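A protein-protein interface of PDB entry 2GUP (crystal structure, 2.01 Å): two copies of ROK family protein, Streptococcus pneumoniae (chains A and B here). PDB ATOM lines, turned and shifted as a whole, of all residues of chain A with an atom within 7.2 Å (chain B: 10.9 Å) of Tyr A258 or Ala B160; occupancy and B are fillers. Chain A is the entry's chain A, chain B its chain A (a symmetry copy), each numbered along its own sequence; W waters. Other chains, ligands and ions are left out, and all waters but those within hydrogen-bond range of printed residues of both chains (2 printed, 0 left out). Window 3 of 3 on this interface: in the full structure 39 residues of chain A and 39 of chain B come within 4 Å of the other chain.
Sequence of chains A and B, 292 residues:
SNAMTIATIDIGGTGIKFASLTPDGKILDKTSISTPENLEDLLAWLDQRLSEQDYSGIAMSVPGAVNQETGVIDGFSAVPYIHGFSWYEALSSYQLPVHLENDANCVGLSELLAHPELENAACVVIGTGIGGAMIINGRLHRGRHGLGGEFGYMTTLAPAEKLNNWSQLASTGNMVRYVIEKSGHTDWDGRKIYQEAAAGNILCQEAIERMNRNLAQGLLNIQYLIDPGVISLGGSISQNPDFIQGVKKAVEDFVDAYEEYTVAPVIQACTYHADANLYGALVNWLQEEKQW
Of the 12 printed residues of chain A, 4 touch a printed residue of chain B. Of the 14 printed residues of chain B, 7 touch a printed residue of chain A. Hydrophobic or aromatic side chains of chain B that line the printed part of chain A: Tyr B153, Pro B159 and Leu B163. Among the printed residues, no Asp or Glu carboxylate lies within 4 Å of a Lys or Arg side-chain nitrogen of the other chain.
Of the printed residues of chain B, Tyr A258 touches Pro B159 (3.4 Å), Ala B160 (2.6 Å), Lys B162 (3.8 Å) and Leu B163 (3.7 Å). Of chain A, only Tyr A258 (2.6 Å) comes within 4 Å of Ala B160. No residue of chain B comes within 4 Å of Ala A257. No residue of chain B comes within 4 Å of Glu A259. Glu A260 touches three residues of chain B. Of the printed residues of chain A, Pro B159 touches Phe A254 and Tyr A258. Printed residues of chain A within 4 Å of Thr B155: Tyr A261. Of the printed residues of chain A, Lys B162 touches Tyr A258 (3.8 Å). Asp A256 touches none of the printed residues of chain B. The nearest residue of chain B that does not touch Tyr A258 is Glu B161 (4.3 Å). The nearest printed residue of chain A that does not touch Tyr B153 is Tyr A261 (4.3 Å).
Water W2 lies within hydrogen-bond range of the backbone carbonyl oxygen (O) of Tyr B153 (2.6 Å) and the side-chain hydroxyl (OH) of Tyr A261 (2.7 Å). Water W1 bridges OH of Tyr A261 (2.6 Å) and OG1 of Thr B155 (3.0 Å).
No position is printed for both chains.
Among the printed residues, pairs that only touch across the chains: Phe A254 with Pro B159 (3.6 Å), Tyr A258 with Pro B159 (3.4 Å), Tyr A258 with Lys B162 (3.8 Å), Tyr A258 with Leu B163 (3.7 Å), Glu A260 with Tyr B153 (3.5 Å), Glu A260 with Leu B163 (3.5 Å), Tyr A261 with Thr B155 (3.7 Å) and Tyr A261 with Leu B163 (3.7 Å).
The backbone carbonyl oxygen (O) of Lys B162 lies within hydrogen-bond range of the side-chain amide nitrogen (ND2) of Asn B164 (3.4 Å). NE2 of Gln B168 lies close to OD1 of Asn B165 (3.2 Å). N of Asn B164 sits at hydrogen-bond distance from OE1 of Gln B168 (2.9 Å).
The side-chain hydroxyl (OH) of Tyr A258 lies within hydrogen-bond range of the backbone carbonyl oxygen (O) of Ala B160 (2.6 Å). The side-chain carboxylate (OE1) of Glu A260 lies within hydrogen-bond range of the side-chain amide nitrogen (NE2) of Gln B168 (3.2 Å).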
ATOM      1  N   LEU A 220     -15.422 -30.295   2.739  1.00  0.00           N
ATOM      2  CA  LEU A 220     -16.838 -30.608   2.883  1.00  0.00           C
ATOM      3  C   LEU A 220     -17.168 -32.034   2.443  1.00  0.00           C
ATOM      4  O   LEU A 220     -18.035 -32.598   3.001  1.00  0.00           O
ATOM      5  CB  LEU A 220     -17.706 -29.586   2.144  1.00  0.00           C
ATOM      6  CG  LEU A 220     -17.768 -28.210   2.781  1.00  0.00           C
ATOM      7  CD1 LEU A 220     -18.169 -27.124   1.704  1.00  0.00           C
ATOM      8  CD2 LEU A 220     -18.818 -28.191   3.885  1.00  0.00           C
ATOM      9  N   GLU A 252     -16.892 -21.520   4.404  1.00  0.00           N
ATOM     10  CA  GLU A 252     -18.082 -20.739   4.787  1.00  0.00           C
ATOM     11  C   GLU A 252     -18.849 -20.290   3.526  1.00  0.00           C
ATOM     12  O   GLU A 252     -20.104 -20.223   3.514  1.00  0.00           O
ATOM     13  CB  GLU A 252     -17.632 -19.563   5.628  1.00  0.00           C
ATOM     14  CG  GLU A 252     -18.454 -19.244   6.905  1.00  0.00           C
ATOM     15  CD  GLU A 252     -18.137 -17.795   7.445  1.00  0.00           C
ATOM     16  OE1 GLU A 252     -16.924 -17.485   7.660  1.00  0.00           O
ATOM     17  OE2 GLU A 252     -19.092 -16.989   7.648  1.00  0.00           O
ATOM     18  N   ASP A 253     -18.138 -19.994   2.455  1.00  0.00           N
ATOM     19  CA  ASP A 253     -18.819 -19.511   1.273  1.00  0.00           C
ATOM     20  C   ASP A 253     -19.620 -20.585   0.523  1.00  0.00           C
ATOM     21  O   ASP A 253     -20.649 -20.282  -0.146  1.00  0.00           O
ATOM     22  CB  ASP A 253     -17.785 -18.996   0.313  1.00  0.00           C
ATOM     23  CG  ASP A 253     -17.288 -17.624   0.639  1.00  0.00           C
ATOM     24  OD1 ASP A 253     -17.793 -16.929   1.573  1.00  0.00           O
ATOM     25  OD2 ASP A 253     -16.330 -17.263  -0.055  1.00  0.00           O
ATOM     26  N   PHE A 254     -19.109 -21.835   0.518  1.00  0.00           N
ATOM     27  CA  PHE A 254     -19.898 -22.995   0.009  1.00  0.00           C
ATOM     28  C   PHE A 254     -21.144 -23.299   0.824  1.00  0.00           C
ATOM     29  O   PHE A 254     -22.189 -23.553   0.268  1.00  0.00           O
ATOM     30  CB  PHE A 254     -19.069 -24.282  -0.007  1.00  0.00           C
ATOM     31  CG  PHE A 254     -18.249 -24.454  -1.234  1.00  0.00           C
ATOM     32  CD1 PHE A 254     -18.852 -24.638  -2.464  1.00  0.00           C
ATOM     33  CD2 PHE A 254     -16.861 -24.426  -1.150  1.00  0.00           C
ATOM     34  CE1 PHE A 254     -18.065 -24.787  -3.625  1.00  0.00           C
ATOM     35  CE2 PHE A 254     -16.073 -24.605  -2.274  1.00  0.00           C
ATOM     36  CZ  PHE A 254     -16.665 -24.761  -3.525  1.00  0.00           C
ATOM     37  N   VAL A 255     -20.977 -23.307   2.153  1.00  0.00           N
ATOM     38  CA  VAL A 255     -22.042 -23.541   3.075  1.00  0.00           C
ATOM     39  C   VAL A 255     -23.187 -22.504   2.880  1.00  0.00           C
ATOM     40  O   VAL A 255     -24.356 -22.864   2.746  1.00  0.00           O
ATOM     41  CB  VAL A 255     -21.482 -23.525   4.535  1.00  0.00           C
ATOM     42  CG1 VAL A 255     -22.592 -23.680   5.573  1.00  0.00           C
ATOM     43  CG2 VAL A 255     -20.449 -24.616   4.731  1.00  0.00           C
ATOM     44  N   ASP A 256     -22.835 -21.221   2.815  1.00  0.00           N
ATOM     45  CA  ASP A 256     -23.849 -20.169   2.658  1.00  0.00           C
ATOM     46  C   ASP A 256     -24.515 -20.282   1.324  1.00  0.00           C
ATOM     47  O   ASP A 256     -25.672 -20.006   1.235  1.00  0.00           O
ATOM     48  CB  ASP A 256     -23.263 -18.764   2.824  1.00  0.00           C
ATOM     49  CG  ASP A 256     -22.789 -18.467   4.279  1.00  0.00           C
ATOM     50  OD1 ASP A 256     -23.141 -19.166   5.312  1.00  0.00           O
ATOM     51  OD2 ASP A 256     -22.005 -17.494   4.363  1.00  0.00           O
ATOM     52  N   ALA A 257     -23.813 -20.733   0.305  1.00  0.00           N
ATOM     53  CA  ALA A 257     -24.413 -20.854  -1.011  1.00  0.00           C
ATOM     54  C   ALA A 257     -25.293 -22.094  -1.249  1.00  0.00           C
ATOM     55  O   ALA A 257     -26.164 -22.090  -2.127  1.00  0.00           O
ATOM     56  CB  ALA A 257     -23.341 -20.798  -2.048  1.00  0.00           C
ATOM     57  N   TYR A 258     -25.076 -23.183  -0.527  1.00  0.00           N
ATOM     58  CA  TYR A 258     -25.851 -24.365  -0.870  1.00  0.00           C
ATOM     59  C   TYR A 258     -26.656 -24.751   0.340  1.00  0.00           C
ATOM     60  O   TYR A 258     -26.105 -24.992   1.413  1.00  0.00           O
ATOM     61  CB  TYR A 258     -24.995 -25.524  -1.497  1.00  0.00           C
ATOM     62  CG  TYR A 258     -24.303 -25.102  -2.778  1.00  0.00           C
ATOM     63  CD1 TYR A 258     -23.047 -24.465  -2.736  1.00  0.00           C
ATOM     64  CD2 TYR A 258     -24.941 -25.192  -4.004  1.00  0.00           C
ATOM     65  CE1 TYR A 258     -22.418 -24.058  -3.841  1.00  0.00           C
ATOM     66  CE2 TYR A 258     -24.296 -24.786  -5.140  1.00  0.00           C
ATOM     67  CZ  TYR A 258     -23.051 -24.208  -5.037  1.00  0.00           C
ATOM     68  OH  TYR A 258     -22.421 -23.742  -6.131  1.00  0.00           O
ATOM     69  N   GLU A 259     -27.982 -24.791   0.150  1.00  0.00           N
ATOM     70  CA  GLU A 259     -28.934 -24.991   1.264  1.00  0.00           C
ATOM     71  C   GLU A 259     -28.771 -26.414   1.802  1.00  0.00           C
ATOM     72  O   GLU A 259     -28.893 -26.645   2.989  1.00  0.00           O
ATOM     73  CB  GLU A 259     -30.388 -24.704   0.788  1.00  0.00           C
ATOM     74  CG  GLU A 259     -31.409 -24.411   1.941  1.00  0.00           C
ATOM     75  CD  GLU A 259     -31.331 -22.978   2.629  1.00  0.00           C
ATOM     76  OE1 GLU A 259     -30.293 -22.241   2.531  1.00  0.00           O
ATOM     77  OE2 GLU A 259     -32.334 -22.610   3.311  1.00  0.00           O
ATOM     78  N   GLU A 260     -28.410 -27.321   0.898  1.00  0.00           N
ATOM     79  CA  GLU A 260     -27.905 -28.641   1.227  1.00  0.00           C
ATOM     80  C   GLU A 260     -26.928 -28.709   2.436  1.00  0.00           C
ATOM     81  O   GLU A 260     -27.048 -29.619   3.220  1.00  0.00           O
ATOM     82  CB  GLU A 260     -27.185 -29.222   0.022  1.00  0.00           C
ATOM     83  CG  GLU A 260     -28.054 -29.784  -1.070  1.00  0.00           C
ATOM     84  CD  GLU A 260     -28.284 -28.764  -2.180  1.00  0.00           C
ATOM     85  OE1 GLU A 260     -28.654 -29.204  -3.295  1.00  0.00           O
ATOM     86  OE2 GLU A 260     -28.054 -27.542  -1.965  1.00  0.00           O
ATOM     87  N   TYR A 261     -25.951 -27.785   2.546  1.00  0.00           N
ATOM     88  CA  TYR A 261     -25.017 -27.755   3.680  1.00  0.00           C
ATOM     89  C   TYR A 261     -25.520 -27.146   4.987  1.00  0.00           C
ATOM     90  O   TYR A 261     -25.937 -25.992   5.044  1.00  0.00           O
ATOM     91  CB  TYR A 261     -23.680 -27.079   3.325  1.00  0.00           C
ATOM     92  CG  TYR A 261     -22.848 -27.850   2.325  1.00  0.00           C
ATOM     93  CD1 TYR A 261     -22.445 -27.238   1.140  1.00  0.00           C
ATOM     94  CD2 TYR A 261     -22.488 -29.215   2.529  1.00  0.00           C
ATOM     95  CE1 TYR A 261     -21.704 -27.930   0.200  1.00  0.00           C
ATOM     96  CE2 TYR A 261     -21.763 -29.895   1.573  1.00  0.00           C
ATOM     97  CZ  TYR A 261     -21.374 -29.233   0.388  1.00  0.00           C
ATOM     98  OH  TYR A 261     -20.596 -29.825  -0.626  1.00  0.00           O
ATOM     99  N   THR A 262     -25.400 -27.920   6.052  1.00  0.00           N
ATOM    100  CA  THR A 262     -25.818 -27.446   7.339  1.00  0.00           C
ATOM    101  C   THR A 262     -24.586 -27.247   8.233  1.00  0.00           C
ATOM    102  O   THR A 262     -24.183 -26.103   8.492  1.00  0.00           O
ATOM    103  CB  THR A 262     -26.858 -28.404   7.988  1.00  0.00           C
ATOM    104  OG1 THR A 262     -27.057 -27.995   9.343  1.00  0.00           O
ATOM    105  CG2 THR A 262     -26.379 -29.897   7.956  1.00  0.00           C
ATOM    106  N   TYR B 153     -23.826 -36.824  -0.280  1.00  0.00           N
ATOM    107  CA  TYR B 153     -23.384 -35.406  -0.241  1.00  0.00           C
ATOM    108  C   TYR B 153     -22.081 -35.123  -1.004  1.00  0.00           C
ATOM    109  O   TYR B 153     -21.666 -33.941  -1.129  1.00  0.00           O
ATOM    110  CB  TYR B 153     -23.211 -34.950   1.190  1.00  0.00           C
ATOM    111  CG  TYR B 153     -24.496 -34.604   1.900  1.00  0.00           C
ATOM    112  CD1 TYR B 153     -25.268 -35.584   2.492  1.00  0.00           C
ATOM    113  CD2 TYR B 153     -24.895 -33.259   2.038  1.00  0.00           C
ATOM    114  CE1 TYR B 153     -26.453 -35.250   3.193  1.00  0.00           C
ATOM    115  CE2 TYR B 153     -26.050 -32.911   2.742  1.00  0.00           C
ATOM    116  CZ  TYR B 153     -26.822 -33.913   3.314  1.00  0.00           C
ATOM    117  OH  TYR B 153     -27.969 -33.550   3.962  1.00  0.00           O
ATOM    118  N   THR B 155     -19.516 -34.197  -3.672  1.00  0.00           N
ATOM    119  CA  THR B 155     -19.553 -33.481  -4.958  1.00  0.00           C
ATOM    120  C   THR B 155     -18.445 -34.008  -5.885  1.00  0.00           C
ATOM    121  O   THR B 155     -17.239 -33.956  -5.589  1.00  0.00           O
ATOM    122  CB  THR B 155     -19.421 -31.966  -4.743  1.00  0.00           C
ATOM    123  OG1 THR B 155     -18.194 -31.686  -4.071  1.00  0.00           O
ATOM    124  CG2 THR B 155     -20.579 -31.424  -3.926  1.00  0.00           C
ATOM    125  N   THR B 156     -18.870 -34.560  -6.992  1.00  0.00           N
ATOM    126  CA  THR B 156     -17.963 -35.165  -7.980  1.00  0.00           C
ATOM    127  C   THR B 156     -17.834 -34.277  -9.194  1.00  0.00           C
ATOM    128  O   THR B 156     -17.211 -34.664 -10.175  1.00  0.00           O
ATOM    129  CB  THR B 156     -18.534 -36.467  -8.466  1.00  0.00           C
ATOM    130  OG1 THR B 156     -19.902 -36.241  -8.888  1.00  0.00           O
ATOM    131  CG2 THR B 156     -18.471 -37.470  -7.386  1.00  0.00           C
ATOM    132  N   LEU B 157     -18.467 -33.115  -9.136  1.00  0.00           N
ATOM    133  CA  LEU B 157     -18.235 -32.050 -10.134  1.00  0.00           C
ATOM    134  C   LEU B 157     -18.081 -30.848  -9.283  1.00  0.00           C
ATOM    135  O   LEU B 157     -18.553 -30.842  -8.179  1.00  0.00           O
ATOM    136  CB  LEU B 157     -19.527 -31.831 -10.991  1.00  0.00           C
ATOM    137  CG  LEU B 157     -19.755 -32.312 -12.417  1.00  0.00           C
ATOM    138  CD1 LEU B 157     -18.924 -33.502 -12.854  1.00  0.00           C
ATOM    139  CD2 LEU B 157     -21.237 -32.562 -12.710  1.00  0.00           C
ATOM    140  N   ALA B 158     -17.549 -29.770  -9.830  1.00  0.00           N
ATOM    141  CA  ALA B 158     -17.552 -28.488  -9.186  1.00  0.00           C
ATOM    142  C   ALA B 158     -18.988 -28.018  -8.949  1.00  0.00           C
ATOM    143  O   ALA B 158     -19.790 -28.121  -9.837  1.00  0.00           O
ATOM    144  CB  ALA B 158     -16.793 -27.466 -10.087  1.00  0.00           C
ATOM    145  N   PRO B 159     -19.334 -27.614  -7.708  1.00  0.00           N
ATOM    146  CA  PRO B 159     -20.617 -26.946  -7.518  1.00  0.00           C
ATOM    147  C   PRO B 159     -20.759 -25.697  -8.408  1.00  0.00           C
ATOM    148  O   PRO B 159     -19.765 -25.019  -8.700  1.00  0.00           O
ATOM    149  CB  PRO B 159     -20.619 -26.568  -6.047  1.00  0.00           C
ATOM    150  CG  PRO B 159     -19.670 -27.502  -5.398  1.00  0.00           C
ATOM    151  CD  PRO B 159     -18.621 -27.841  -6.439  1.00  0.00           C
ATOM    152  N   ALA B 160     -21.990 -25.453  -8.875  1.00  0.00           N
ATOM    153  CA  ALA B 160     -22.296 -24.319  -9.724  1.00  0.00           C
ATOM    154  C   ALA B 160     -23.711 -23.870  -9.383  1.00  0.00           C
ATOM    155  O   ALA B 160     -24.039 -23.629  -8.218  1.00  0.00           O
ATOM    156  CB  ALA B 160     -22.157 -24.687 -11.286  1.00  0.00           C
ATOM    157  N   GLU B 161     -24.561 -23.812 -10.395  1.00  0.00           N
ATOM    158  CA  GLU B 161     -25.938 -23.461 -10.170  1.00  0.00           C
ATOM    159  C   GLU B 161     -26.489 -24.482  -9.208  1.00  0.00           C
ATOM    160  O   GLU B 161     -27.185 -24.112  -8.265  1.00  0.00           O
ATOM    161  CB  GLU B 161     -26.722 -23.408 -11.492  1.00  0.00           C
ATOM    162  CG  GLU B 161     -26.100 -22.440 -12.573  1.00  0.00           C
ATOM    163  CD  GLU B 161     -26.051 -20.937 -12.145  1.00  0.00           C
ATOM    164  OE1 GLU B 161     -26.978 -20.161 -12.524  1.00  0.00           O
ATOM    165  OE2 GLU B 161     -25.073 -20.521 -11.448  1.00  0.00           O
ATOM    166  N   LYS B 162     -26.116 -25.748  -9.414  1.00  0.00           N
ATOM    167  CA  LYS B 162     -26.546 -26.847  -8.549  1.00  0.00           C
ATOM    168  C   LYS B 162     -25.330 -27.356  -7.762  1.00  0.00           C
ATOM    169  O   LYS B 162     -24.185 -27.117  -8.136  1.00  0.00           O
ATOM    170  CB  LYS B 162     -27.188 -27.949  -9.376  1.00  0.00           C
ATOM    171  CG  LYS B 162     -28.679 -27.657  -9.654  1.00  0.00           C
ATOM    172  CD  LYS B 162     -29.414 -28.820 -10.315  1.00  0.00           C
ATOM    173  CE  LYS B 162     -28.628 -29.374 -11.529  1.00  0.00           C
ATOM    174  NZ  LYS B 162     -29.231 -29.135 -12.965  1.00  0.00           N
ATOM    175  N   LEU B 163     -25.585 -28.026  -6.657  1.00  0.00           N
ATOM    176  CA  LEU B 163     -24.533 -28.481  -5.834  1.00  0.00           C
ATOM    177  C   LEU B 163     -23.713 -29.528  -6.598  1.00  0.00           C
ATOM    178  O   LEU B 163     -22.492 -29.573  -6.465  1.00  0.00           O
ATOM    179  CB  LEU B 163     -25.074 -29.003  -4.536  1.00  0.00           C
ATOM    180  CG  LEU B 163     -23.971 -29.532  -3.602  1.00  0.00           C
ATOM    181  CD1 LEU B 163     -22.848 -28.512  -3.286  1.00  0.00           C
ATOM    182  CD2 LEU B 163     -24.648 -29.877  -2.358  1.00  0.00           C
ATOM    183  N   ASN B 164     -24.355 -30.270  -7.485  1.00  0.00           N
ATOM    184  CA  ASN B 164     -23.687 -31.370  -8.145  1.00  0.00           C
ATOM    185  C   ASN B 164     -23.134 -32.438  -7.169  1.00  0.00           C
ATOM    186  O   ASN B 164     -22.061 -32.985  -7.429  1.00  0.00           O
ATOM    187  CB  ASN B 164     -22.574 -30.824  -9.030  1.00  0.00           C
ATOM    188  CG  ASN B 164     -23.126 -29.963 -10.174  1.00  0.00           C
ATOM    189  OD1 ASN B 164     -24.213 -30.256 -10.723  1.00  0.00           O
ATOM    190  ND2 ASN B 164     -22.418 -28.890 -10.496  1.00  0.00           N
ATOM    191  N   ASN B 165     -23.846 -32.685  -6.052  1.00  0.00           N
ATOM    192  CA  ASN B 165     -23.561 -33.826  -5.156  1.00  0.00           C
ATOM    193  C   ASN B 165     -23.947 -35.158  -5.818  1.00  0.00           C
ATOM    194  O   ASN B 165     -24.799 -35.218  -6.773  1.00  0.00           O
ATOM    195  CB  ASN B 165     -24.236 -33.647  -3.753  1.00  0.00           C
ATOM    196  CG  ASN B 165     -25.768 -33.468  -3.837  1.00  0.00           C
ATOM    197  OD1 ASN B 165     -26.237 -32.646  -4.601  1.00  0.00           O
ATOM    198  ND2 ASN B 165     -26.539 -34.201  -3.033  1.00  0.00           N
ATOM    199  N   GLN B 168     -27.560 -36.256  -6.592  1.00  0.00           N
ATOM    200  CA  GLN B 168     -28.029 -35.594  -7.800  1.00  0.00           C
ATOM    201  C   GLN B 168     -27.561 -36.216  -9.095  1.00  0.00           C
ATOM    202  O   GLN B 168     -28.265 -36.143 -10.096  1.00  0.00           O
ATOM    203  CB  GLN B 168     -27.624 -34.102  -7.817  1.00  0.00           C
ATOM    204  CG  GLN B 168     -28.489 -33.161  -7.017  1.00  0.00           C
ATOM    205  CD  GLN B 168     -27.910 -31.712  -6.968  1.00  0.00           C
ATOM    206  OE1 GLN B 168     -26.984 -31.364  -7.733  1.00  0.00           O
ATOM    207  NE2 GLN B 168     -28.452 -30.876  -6.043  1.00  0.00           N
ATOM    208  N   LEU B 169     -26.373 -36.808  -9.140  1.00  0.00           N
ATOM    209  CA  LEU B 169     -25.859 -37.215 -10.416  1.00  0.00           C
ATOM    210  C   LEU B 169     -25.968 -38.680 -10.628  1.00  0.00           C
ATOM    211  O   LEU B 169     -25.910 -39.140 -11.802  1.00  0.00           O
ATOM    212  CB  LEU B 169     -24.374 -36.812 -10.564  1.00  0.00           C
ATOM    213  CG  LEU B 169     -24.105 -35.306 -10.445  1.00  0.00           C
ATOM    214  CD1 LEU B 169     -22.642 -34.968 -10.115  1.00  0.00           C
ATOM    215  CD2 LEU B 169     -24.588 -34.618 -11.782  1.00  0.00           C
HETATM  216  O   HOH W   1     -18.212 -29.914  -1.688  1.00  0.00           O
HETATM  217  O   HOH W   2     -20.069 -32.349   0.112  1.00  0.00           O
